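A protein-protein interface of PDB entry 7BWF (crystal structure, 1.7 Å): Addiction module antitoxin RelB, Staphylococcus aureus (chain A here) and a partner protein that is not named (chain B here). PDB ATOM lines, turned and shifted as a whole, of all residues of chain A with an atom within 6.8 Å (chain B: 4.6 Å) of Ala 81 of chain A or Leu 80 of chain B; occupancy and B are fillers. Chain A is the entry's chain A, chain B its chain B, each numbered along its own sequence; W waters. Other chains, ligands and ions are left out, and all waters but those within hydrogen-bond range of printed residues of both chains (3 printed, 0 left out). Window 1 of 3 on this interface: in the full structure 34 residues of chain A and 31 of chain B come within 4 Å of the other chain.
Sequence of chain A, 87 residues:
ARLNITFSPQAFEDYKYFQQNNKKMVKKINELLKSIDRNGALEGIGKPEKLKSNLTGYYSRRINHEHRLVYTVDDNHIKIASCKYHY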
ATOM      1  N   THR A   6     -32.272   0.192  23.849  1.00  0.00           N
ATOM      2  CA  THR A   6     -32.623  -1.219  23.809  1.00  0.00           C
ATOM      3  C   THR A   6     -31.538  -1.990  23.062  1.00  0.00           C
ATOM      4  O   THR A   6     -31.203  -1.644  21.924  1.00  0.00           O
ATOM      5  CB  THR A   6     -33.975  -1.429  23.131  1.00  0.00           C
ATOM      6  OG1 THR A   6     -35.014  -0.899  23.962  1.00  0.00           O
ATOM      7  CG2 THR A   6     -34.218  -2.901  22.912  1.00  0.00           C
ATOM      8  N   PHE A   7     -30.979  -3.014  23.718  1.00  0.00           N
ATOM      9  CA  PHE A   7     -29.941  -3.866  23.144  1.00  0.00           C
ATOM     10  C   PHE A   7     -30.494  -5.235  22.760  1.00  0.00           C
ATOM     11  O   PHE A   7     -31.372  -5.777  23.439  1.00  0.00           O
ATOM     12  CB  PHE A   7     -28.769  -4.142  24.135  1.00  0.00           C
ATOM     13  CG  PHE A   7     -27.918  -2.944  24.448  1.00  0.00           C
ATOM     14  CD1 PHE A   7     -28.286  -2.075  25.460  1.00  0.00           C
ATOM     15  CD2 PHE A   7     -26.734  -2.703  23.765  1.00  0.00           C
ATOM     16  CE1 PHE A   7     -27.514  -0.967  25.765  1.00  0.00           C
ATOM     17  CE2 PHE A   7     -25.950  -1.594  24.073  1.00  0.00           C
ATOM     18  CZ  PHE A   7     -26.346  -0.727  25.075  1.00  0.00           C
ATOM     19  N   SER A   8     -29.926  -5.825  21.705  1.00  0.00           N
ATOM     20  CA  SER A   8     -30.021  -7.266  21.527  1.00  0.00           C
ATOM     21  C   SER A   8     -29.111  -7.939  22.557  1.00  0.00           C
ATOM     22  O   SER A   8     -28.126  -7.338  23.004  1.00  0.00           O
ATOM     23  CB  SER A   8     -29.600  -7.685  20.116  1.00  0.00           C
ATOM     24  OG  SER A   8     -28.225  -7.424  19.892  1.00  0.00           O
ATOM     25  N   PRO A   9     -29.424  -9.177  22.965  1.00  0.00           N
ATOM     26  CA  PRO A   9     -28.542  -9.860  23.932  1.00  0.00           C
ATOM     27  C   PRO A   9     -27.066  -9.833  23.543  1.00  0.00           C
ATOM     28  O   PRO A   9     -26.209  -9.547  24.386  1.00  0.00           O
ATOM     29  CB  PRO A   9     -29.114 -11.283  23.959  1.00  0.00           C
ATOM     30  CG  PRO A   9     -30.597 -11.053  23.777  1.00  0.00           C
ATOM     31  CD  PRO A   9     -30.693  -9.912  22.766  1.00  0.00           C
ATOM     32  N   GLN A  10     -26.737 -10.131  22.286  1.00  0.00           N
ATOM     33  CA  GLN A  10     -25.331 -10.221  21.906  1.00  0.00           C
ATOM     34  C   GLN A  10     -24.697  -8.838  21.837  1.00  0.00           C
ATOM     35  O   GLN A  10     -23.531  -8.665  22.204  1.00  0.00           O
ATOM     36  CB  GLN A  10     -25.184 -10.959  20.570  1.00  0.00           C
ATOM     37  CG  GLN A  10     -25.511 -12.449  20.644  1.00  0.00           C
ATOM     38  CD  GLN A  10     -25.624 -13.074  19.267  1.00  0.00           C
ATOM     39  OE1 GLN A  10     -24.803 -12.809  18.387  1.00  0.00           O
ATOM     40  NE2 GLN A  10     -26.646 -13.897  19.069  1.00  0.00           N
ATOM     41  N   ALA A  11     -25.448  -7.839  21.373  1.00  0.00           N
ATOM     42  CA  ALA A  11     -24.930  -6.475  21.353  1.00  0.00           C
ATOM     43  C   ALA A  11     -24.636  -5.981  22.768  1.00  0.00           C
ATOM     44  O   ALA A  11     -23.657  -5.263  22.991  1.00  0.00           O
ATOM     45  CB  ALA A  11     -25.920  -5.546  20.639  1.00  0.00           C
ATOM     46  N   PHE A  12     -25.461  -6.367  23.743  1.00  0.00           N
ATOM     47  CA  PHE A  12     -25.199  -5.950  25.117  1.00  0.00           C
ATOM     48  C   PHE A  12     -23.909  -6.565  25.640  1.00  0.00           C
ATOM     49  O   PHE A  12     -23.089  -5.884  26.260  1.00  0.00           O
ATOM     50  CB  PHE A  12     -26.350  -6.333  26.036  1.00  0.00           C
ATOM     51  CG  PHE A  12     -26.267  -5.679  27.376  1.00  0.00           C
ATOM     52  CD1 PHE A  12     -26.143  -4.302  27.477  1.00  0.00           C
ATOM     53  CD2 PHE A  12     -26.282  -6.432  28.531  1.00  0.00           C
ATOM     54  CE1 PHE A  12     -26.060  -3.693  28.710  1.00  0.00           C
ATOM     55  CE2 PHE A  12     -26.204  -5.826  29.769  1.00  0.00           C
ATOM     56  CZ  PHE A  12     -26.087  -4.457  29.858  1.00  0.00           C
ATOM     57  N   ASP A  14     -21.316  -7.386  24.007  1.00  0.00           N
ATOM     58  CA  ASP A  14     -20.197  -6.677  23.388  1.00  0.00           C
ATOM     59  C   ASP A  14     -20.044  -5.275  23.968  1.00  0.00           C
ATOM     60  O   ASP A  14     -18.924  -4.823  24.231  1.00  0.00           O
ATOM     61  CB  ASP A  14     -20.396  -6.616  21.866  1.00  0.00           C
ATOM     62  CG  ASP A  14     -20.365  -8.002  21.204  1.00  0.00           C
ATOM     63  OD1 ASP A  14     -19.645  -8.894  21.699  1.00  0.00           O
ATOM     64  OD2 ASP A  14     -21.056  -8.207  20.190  1.00  0.00           O
ATOM     65  N   TYR A  58     -32.709  -1.500   9.026  1.00  0.00           N
ATOM     66  CA  TYR A  58     -31.634  -1.133   9.926  1.00  0.00           C
ATOM     67  C   TYR A  58     -30.629  -0.232   9.231  1.00  0.00           C
ATOM     68  O   TYR A  58     -30.648  -0.038   8.016  1.00  0.00           O
ATOM     69  CB  TYR A  58     -30.951  -2.383  10.477  1.00  0.00           C
ATOM     70  CG  TYR A  58     -31.765  -3.031  11.569  1.00  0.00           C
ATOM     71  CD1 TYR A  58     -32.909  -3.757  11.266  1.00  0.00           C
ATOM     72  CD2 TYR A  58     -31.406  -2.903  12.903  1.00  0.00           C
ATOM     73  CE1 TYR A  58     -33.665  -4.342  12.262  1.00  0.00           C
ATOM     74  CE2 TYR A  58     -32.156  -3.490  13.904  1.00  0.00           C
ATOM     75  CZ  TYR A  58     -33.286  -4.204  13.577  1.00  0.00           C
ATOM     76  OH  TYR A  58     -34.030  -4.785  14.578  1.00  0.00           O
ATOM     77  N   LEU A  69     -21.796  -0.011  14.240  1.00  0.00           N
ATOM     78  CA  LEU A  69     -23.015   0.084  15.031  1.00  0.00           C
ATOM     79  C   LEU A  69     -24.187  -0.161  14.092  1.00  0.00           C
ATOM     80  O   LEU A  69     -24.441   0.641  13.188  1.00  0.00           O
ATOM     81  CB  LEU A  69     -23.119   1.450  15.699  1.00  0.00           C
ATOM     82  CG  LEU A  69     -24.300   1.645  16.647  1.00  0.00           C
ATOM     83  CD1 LEU A  69     -24.128   0.794  17.906  1.00  0.00           C
ATOM     84  CD2 LEU A  69     -24.465   3.122  17.005  1.00  0.00           C
ATOM     85  N   VAL A  70     -24.881  -1.276  14.291  1.00  0.00           N
ATOM     86  CA  VAL A  70     -26.046  -1.642  13.495  1.00  0.00           C
ATOM     87  C   VAL A  70     -27.289  -1.435  14.352  1.00  0.00           C
ATOM     88  O   VAL A  70     -27.443  -2.074  15.401  1.00  0.00           O
ATOM     89  CB  VAL A  70     -25.951  -3.095  13.007  1.00  0.00           C
ATOM     90  CG1 VAL A  70     -27.137  -3.422  12.141  1.00  0.00           C
ATOM     91  CG2 VAL A  70     -24.641  -3.324  12.260  1.00  0.00           C
ATOM     92  N   TYR A  71     -28.186  -0.560  13.902  1.00  0.00           N
ATOM     93  CA  TYR A  71     -29.269  -0.088  14.750  1.00  0.00           C
ATOM     94  C   TYR A  71     -30.495   0.248  13.912  1.00  0.00           C
ATOM     95  O   TYR A  71     -30.448   0.314  12.683  1.00  0.00           O
ATOM     96  CB  TYR A  71     -28.844   1.157  15.532  1.00  0.00           C
ATOM     97  CG  TYR A  71     -28.529   2.305  14.594  1.00  0.00           C
ATOM     98  CD1 TYR A  71     -27.296   2.392  13.959  1.00  0.00           C
ATOM     99  CD2 TYR A  71     -29.477   3.277  14.305  1.00  0.00           C
ATOM    100  CE1 TYR A  71     -27.010   3.424  13.082  1.00  0.00           C
ATOM    101  CE2 TYR A  71     -29.193   4.318  13.435  1.00  0.00           C
ATOM    102  CZ  TYR A  71     -27.961   4.390  12.829  1.00  0.00           C
ATOM    103  OH  TYR A  71     -27.677   5.419  11.957  1.00  0.00           O
ATOM    104  N   THR A  72     -31.598   0.487  14.617  1.00  0.00           N
ATOM    105  CA  THR A  72     -32.819   1.025  14.040  1.00  0.00           C
ATOM    106  C   THR A  72     -33.464   1.950  15.065  1.00  0.00           C
ATOM    107  O   THR A  72     -33.062   1.999  16.233  1.00  0.00           O
ATOM    108  CB  THR A  72     -33.789  -0.089  13.623  1.00  0.00           C
ATOM    109  OG1 THR A  72     -34.759   0.443  12.711  1.00  0.00           O
ATOM    110  CG2 THR A  72     -34.495  -0.661  14.834  1.00  0.00           C
ATOM    111  N   LYS A  79     -32.651   1.180  19.004  1.00  0.00           N
ATOM    112  CA  LYS A  79     -32.431  -0.236  19.256  1.00  0.00           C
ATOM    113  C   LYS A  79     -31.154  -0.663  18.553  1.00  0.00           C
ATOM    114  O   LYS A  79     -30.965  -0.355  17.369  1.00  0.00           O
ATOM    115  CB  LYS A  79     -33.611  -1.063  18.749  1.00  0.00           C
ATOM    116  CG  LYS A  79     -34.939  -0.582  19.293  1.00  0.00           C
ATOM    117  CD  LYS A  79     -36.000  -1.668  19.256  1.00  0.00           C
ATOM    118  CE  LYS A  79     -37.325  -1.130  19.781  1.00  0.00           C
ATOM    119  NZ  LYS A  79     -38.385  -2.173  19.832  1.00  0.00           N
ATOM    120  N   ILE A  80     -30.305  -1.398  19.268  1.00  0.00           N
ATOM    121  CA  ILE A  80     -28.990  -1.786  18.774  1.00  0.00           C
ATOM    122  C   ILE A  80     -28.994  -3.280  18.518  1.00  0.00           C
ATOM    123  O   ILE A  80     -29.199  -4.083  19.442  1.00  0.00           O
ATOM    124  CB  ILE A  80     -27.874  -1.417  19.762  1.00  0.00           C
ATOM    125  CG1 ILE A  80     -27.824   0.097  19.967  1.00  0.00           C
ATOM    126  CG2 ILE A  80     -26.545  -1.912  19.274  1.00  0.00           C
ATOM    127  CD1 ILE A  80     -26.915   0.549  21.115  1.00  0.00           C
ATOM    128  N   ALA A  81     -28.752  -3.647  17.263  1.00  0.00           N
ATOM    129  CA  ALA A  81     -28.568  -5.042  16.894  1.00  0.00           C
ATOM    130  C   ALA A  81     -27.137  -5.517  17.127  1.00  0.00           C
ATOM    131  O   ALA A  81     -26.928  -6.663  17.542  1.00  0.00           O
ATOM    132  CB  ALA A  81     -28.949  -5.255  15.427  1.00  0.00           C
ATOM    133  N   SER A  82     -26.152  -4.659  16.872  1.00  0.00           N
ATOM    134  CA  SER A  82     -24.750  -5.045  16.943  1.00  0.00           C
ATOM    135  C   SER A  82     -23.904  -3.808  17.193  1.00  0.00           C
ATOM    136  O   SER A  82     -24.258  -2.699  16.782  1.00  0.00           O
ATOM    137  CB  SER A  82     -24.282  -5.728  15.649  1.00  0.00           C
ATOM    138  OG  SER A  82     -22.920  -6.128  15.731  1.00  0.00           O
ATOM    139  N   CYS A  83     -22.762  -4.013  17.856  1.00  0.00           N
ATOM    140  CA  CYS A  83     -21.778  -2.950  18.024  1.00  0.00           C
ATOM    141  C   CYS A  83     -20.361  -3.505  17.919  1.00  0.00           C
ATOM    142  O   CYS A  83     -19.414  -2.872  18.402  1.00  0.00           O
ATOM    143  CB  CYS A  83     -21.962  -2.209  19.366  1.00  0.00           C
ATOM    144  SG  CYS A  83     -21.675  -3.193  20.856  1.00  0.00           S
ATOM    145  N   HIS B  72     -24.946 -13.585  13.563  1.00  0.00           N
ATOM    146  CA  HIS B  72     -25.072 -12.704  14.721  1.00  0.00           C
ATOM    147  C   HIS B  72     -26.090 -11.597  14.447  1.00  0.00           C
ATOM    148  O   HIS B  72     -26.955 -11.313  15.282  1.00  0.00           O
ATOM    149  CB  HIS B  72     -23.682 -12.150  15.073  1.00  0.00           C
ATOM    150  CG  HIS B  72     -23.696 -10.807  15.736  1.00  0.00           C
ATOM    151  ND1 HIS B  72     -24.211 -10.601  17.000  1.00  0.00           N
ATOM    152  CD2 HIS B  72     -23.229  -9.607  15.318  1.00  0.00           C
ATOM    153  CE1 HIS B  72     -24.079  -9.326  17.321  1.00  0.00           C
ATOM    154  NE2 HIS B  72     -23.486  -8.702  16.318  1.00  0.00           N
ATOM    155  N   SER B  76     -29.756 -11.341  16.153  1.00  0.00           N
ATOM    156  CA  SER B  76     -29.973 -10.157  16.978  1.00  0.00           C
ATOM    157  C   SER B  76     -31.198  -9.379  16.512  1.00  0.00           C
ATOM    158  O   SER B  76     -31.966  -8.873  17.335  1.00  0.00           O
ATOM    159  CB  SER B  76     -28.730  -9.256  16.956  1.00  0.00           C
ATOM    160  OG  SER B  76     -27.645  -9.864  17.631  1.00  0.00           O
ATOM    161  N   ILE B  77     -31.400  -9.272  15.197  1.00  0.00           N
ATOM    162  CA  ILE B  77     -32.578  -8.582  14.683  1.00  0.00           C
ATOM    163  C   ILE B  77     -33.836  -9.383  15.003  1.00  0.00           C
ATOM    164  O   ILE B  77     -34.901  -8.814  15.270  1.00  0.00           O
ATOM    165  CB  ILE B  77     -32.430  -8.315  13.172  1.00  0.00           C
ATOM    166  CG1 ILE B  77     -31.369  -7.231  12.951  1.00  0.00           C
ATOM    167  CG2 ILE B  77     -33.774  -7.903  12.586  1.00  0.00           C
ATOM    168  CD1 ILE B  77     -31.001  -6.986  11.499  1.00  0.00           C
ATOM    169  N   ALA B  78     -33.735 -10.712  14.993  1.00  0.00           N
ATOM    170  CA  ALA B  78     -34.867 -11.537  15.410  1.00  0.00           C
ATOM    171  C   ALA B  78     -35.174 -11.315  16.888  1.00  0.00           C
ATOM    172  O   ALA B  78     -36.337 -11.182  17.279  1.00  0.00           O
ATOM    173  CB  ALA B  78     -34.584 -13.019  15.132  1.00  0.00           C
ATOM    174  N   ASP B  79     -34.137 -11.266  17.728  1.00  0.00           N
ATOM    175  CA  ASP B  79     -34.344 -11.019  19.150  1.00  0.00           C
ATOM    176  C   ASP B  79     -35.077  -9.703  19.365  1.00  0.00           C
ATOM    177  O   ASP B  79     -36.062  -9.640  20.107  1.00  0.00           O
ATOM    178  CB  ASP B  79     -33.000 -10.999  19.885  1.00  0.00           C
ATOM    179  CG  ASP B  79     -32.389 -12.379  20.038  1.00  0.00           C
ATOM    180  OD1 ASP B  79     -33.114 -13.386  19.902  1.00  0.00           O
ATOM    181  OD2 ASP B  79     -31.172 -12.450  20.284  1.00  0.00           O
ATOM    182  N   LEU B  80     -34.605  -8.636  18.719  1.00  0.00           N
ATOM    183  CA  LEU B  80     -35.204  -7.320  18.912  1.00  0.00           C
ATOM    184  C   LEU B  80     -36.672  -7.321  18.498  1.00  0.00           C
ATOM    185  O   LEU B  80     -37.511  -6.687  19.146  1.00  0.00           O
ATOM    186  CB  LEU B  80     -34.421  -6.276  18.112  1.00  0.00           C
ATOM    187  CG  LEU B  80     -33.039  -5.879  18.628  1.00  0.00           C
ATOM    188  CD1 LEU B  80     -32.238  -5.211  17.516  1.00  0.00           C
ATOM    189  CD2 LEU B  80     -33.191  -4.965  19.830  1.00  0.00           C
ATOM    190  N   GLU B  81     -37.004  -8.044  17.429  1.00  0.00           N
ATOM    191  CA  GLU B  81     -38.383  -8.070  16.957  1.00  0.00           C
ATOM    192  C   GLU B  81     -39.289  -8.820  17.925  1.00  0.00           C
ATOM    193  O   GLU B  81     -40.483  -8.515  18.018  1.00  0.00           O
ATOM    194  CB  GLU B  81     -38.448  -8.710  15.568  1.00  0.00           C
ATOM    195  CG  GLU B  81     -39.689  -8.361  14.777  1.00  0.00           C
ATOM    196  CD  GLU B  81     -39.583  -8.830  13.334  1.00  0.00           C
ATOM    197  OE1 GLU B  81     -39.085  -8.056  12.496  1.00  0.00           O
ATOM    198  OE2 GLU B  81     -40.000  -9.970  13.037  1.00  0.00           O
ATOM    199  N   ARG B  82     -38.748  -9.785  18.664  1.00  0.00           N
ATOM    200  CA  ARG B  82     -39.548 -10.590  19.581  1.00  0.00           C
ATOM    201  C   ARG B  82     -39.490 -10.086  21.016  1.00  0.00           C
ATOM    202  O   ARG B  82     -40.069 -10.716  21.909  1.00  0.00           O
ATOM    203  CB  ARG B  82     -39.090 -12.049  19.549  1.00  0.00           C
ATOM    204  CG  ARG B  82     -39.038 -12.615  18.158  1.00  0.00           C
ATOM    205  CD  ARG B  82     -38.764 -14.102  18.119  1.00  0.00           C
ATOM    206  NE  ARG B  82     -39.293 -14.628  16.869  1.00  0.00           N
ATOM    207  CZ  ARG B  82     -38.838 -14.282  15.669  1.00  0.00           C
ATOM    208  NH1 ARG B  82     -37.832 -13.421  15.555  1.00  0.00           N
ATOM    209  NH2 ARG B  82     -39.390 -14.795  14.581  1.00  0.00           N
ATOM    210  N   GLY B  83     -38.799  -8.981  21.265  1.00  0.00           N
ATOM    211  CA  GLY B  83     -38.709  -8.442  22.604  1.00  0.00           C
ATOM    212  C   GLY B  83     -37.765  -9.165  23.540  1.00  0.00           C
ATOM    213  O   GLY B  83     -37.771  -8.871  24.743  1.00  0.00           O
ATOM    214  N   THR B  85     -34.822  -8.799  24.721  1.00  0.00           N
ATOM    215  CA  THR B  85     -33.939  -7.647  24.676  1.00  0.00           C
ATOM    216  C   THR B  85     -33.470  -7.274  26.073  1.00  0.00           C
ATOM    217  O   THR B  85     -33.982  -7.759  27.089  1.00  0.00           O
ATOM    218  CB  THR B  85     -34.629  -6.428  24.036  1.00  0.00           C
ATOM    219  OG1 THR B  85     -35.752  -6.036  24.837  1.00  0.00           O
ATOM    220  CG2 THR B  85     -35.086  -6.749  22.625  1.00  0.00           C
HETATM  221  O   HOH W   1     -22.574  -6.787  18.666  1.00  0.00           O
HETATM  222  O   HOH W   2     -35.977  -6.316  14.270  1.00  0.00           O
HETATM  223  O   HOH W   3     -28.737 -10.897  20.189  1.00  0.00           O
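The side-chain hydroxyl of Ser 8 of chain A lies within hydrogen-bond range of the side-chain hydroxyl of Ser 76 of chain B. A ring nitrogen (ND1) of His 72 of chain B is in hydrogen-bond range of the side-chain amide oxygen of Gln 10 of chain A (2.7 Å). O of Ala 81 of chain A lies close to OG of Ser 76 of chain B, at 3.3 Å. The side-chain hydroxyl (OG) of Ser 82 of chain A is in hydrogen-bond range of a ring nitrogen (NE2) of His 72 of chain B, at 2.7 Å.
Water W2 bridges the side-chain hydroxyl (OH) of Tyr 58 of chain A (2.5 Å) and the backbone carbonyl oxygen (O) of Ile 77 of chain B (2.9 Å). Water W1 lies within hydrogen-bond range of OD2 of Asp 14 of chain A (2.6 Å), N of Cys 83 of chain A (2.9 Å), OG of Ser 82 of chain A (3.0 Å) and NE2 of His 72 of chain B (3.2 Å). Water W3 lies within hydrogen-bond range of OD2 of Asp 79 of chain B (2.9 Å), OG of Ser 76 of chain B (3.0 Å) and N of Gln 10 of chain A (3.0 Å).
CD2 of Leu 80 of chain B touches CG2 of Thr 6 of chain A, 3.8 Å away. Thr 6 of chain A touches Thr 85 of chain B (CG2 to CB, 3.7 Å). Phe 7 of chain A touches Thr 85 of chain B (O to CB, 3.4 Å). Ser 8 of chain A touches Leu 80 of chain B (N to CD2, 3.9 Å). Pro 9 of chain A touches Asp 79 of chain B. Gln 10 of chain A touches Ser 76 of chain B. CD1 of Leu 80 of chain B touches OH of Tyr 58 of chain A, 3.5 Å away. Ile 80 of chain A touches Leu 80 of chain B (O to CD1, 3.8 Å). His 72 of chain B touches Ala 81 of chain A (CE1 to O, 3.9 Å). CB of Ala 81 of chain A touches CG1 of Ile 77 of chain B (3.99 Å).
The side-chain hydroxyl (OG) of Ser 8 of chain A sits close to the backbone NH (N) of Ala 11 of chain A (3.2 Å). The backbone NH of Ser 8 of chain A lies within hydrogen-bond range of the backbone carbonyl oxygen of Ile 80 of chain A, at 2.9 Å. The side-chain hydroxyl (OG) of Ser 8 of chain A is in hydrogen-bond range of the backbone carbonyl oxygen (O) of Ala 81 of chain A, 2.8 Å away. N of Val 70 of chain A lies within hydrogen-bond range of O of Ser 82 of chain A (2.9 Å). O of His 72 of chain B sits at hydrogen-bond distance from OG of Ser 76 of chain B (2.8 Å). The side-chain hydroxyl of Thr 85 of chain B lies within hydrogen-bond range of the backbone carbonyl oxygen of Gly 83 of chain B (3.5 Å).
Of the printed residues of chain B, Ser 8 of chain A touches Ser 76 and Leu 80. Printed residues of chain B within 4 Å of Gln 10 of chain A: His 72 (2.7 Å) and Ser 76 (3.99 Å). Of the printed residues of chain B, Tyr 58 of chain A touches Ile 77 (3.6 Å) and Leu 80 (3.5 Å). Lys 79 of chain A touches none of the printed residues of chain B. Of the printed residues of chain A, Leu 80 of chain B touches Thr 6 (3.8 Å), Phe 7 (3.99 Å), Ser 8 (3.9 Å), Tyr 58 (3.5 Å), Ile 80 (3.8 Å) and Ala 81 (3.7 Å). The nearest printed residue of chain B that does not touch Ala 81 of chain A is Ala 78 of chain B (7.3 Å). The nearest printed residue of chain A that does not touch Leu 80 of chain B is Lys 79 of chain A (4.1 Å).
Of the 18 printed residues of chain A, 9 touch a printed residue of chain B. Printed residues of chain A that touch a printed residue of chain B: Thr 6, Phe 7, Ser 8, Pro 9, Gln 10, Tyr 58, Ile 80, Ala 81 and Ser 82. Hydrophobic or aromatic side chains of chain A that line the printed part of chain B: Pro 9, Tyr 58 and Ala 81. Of the 10 printed residues of chain B, 6 touch a printed residue of chain A. Among the printed residues, 17 pairs touch across the chains. Among the printed residues, no Asp or Glu carboxylate lies within 4 Å of a Lys or Arg side-chain nitrogen of the other chain.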
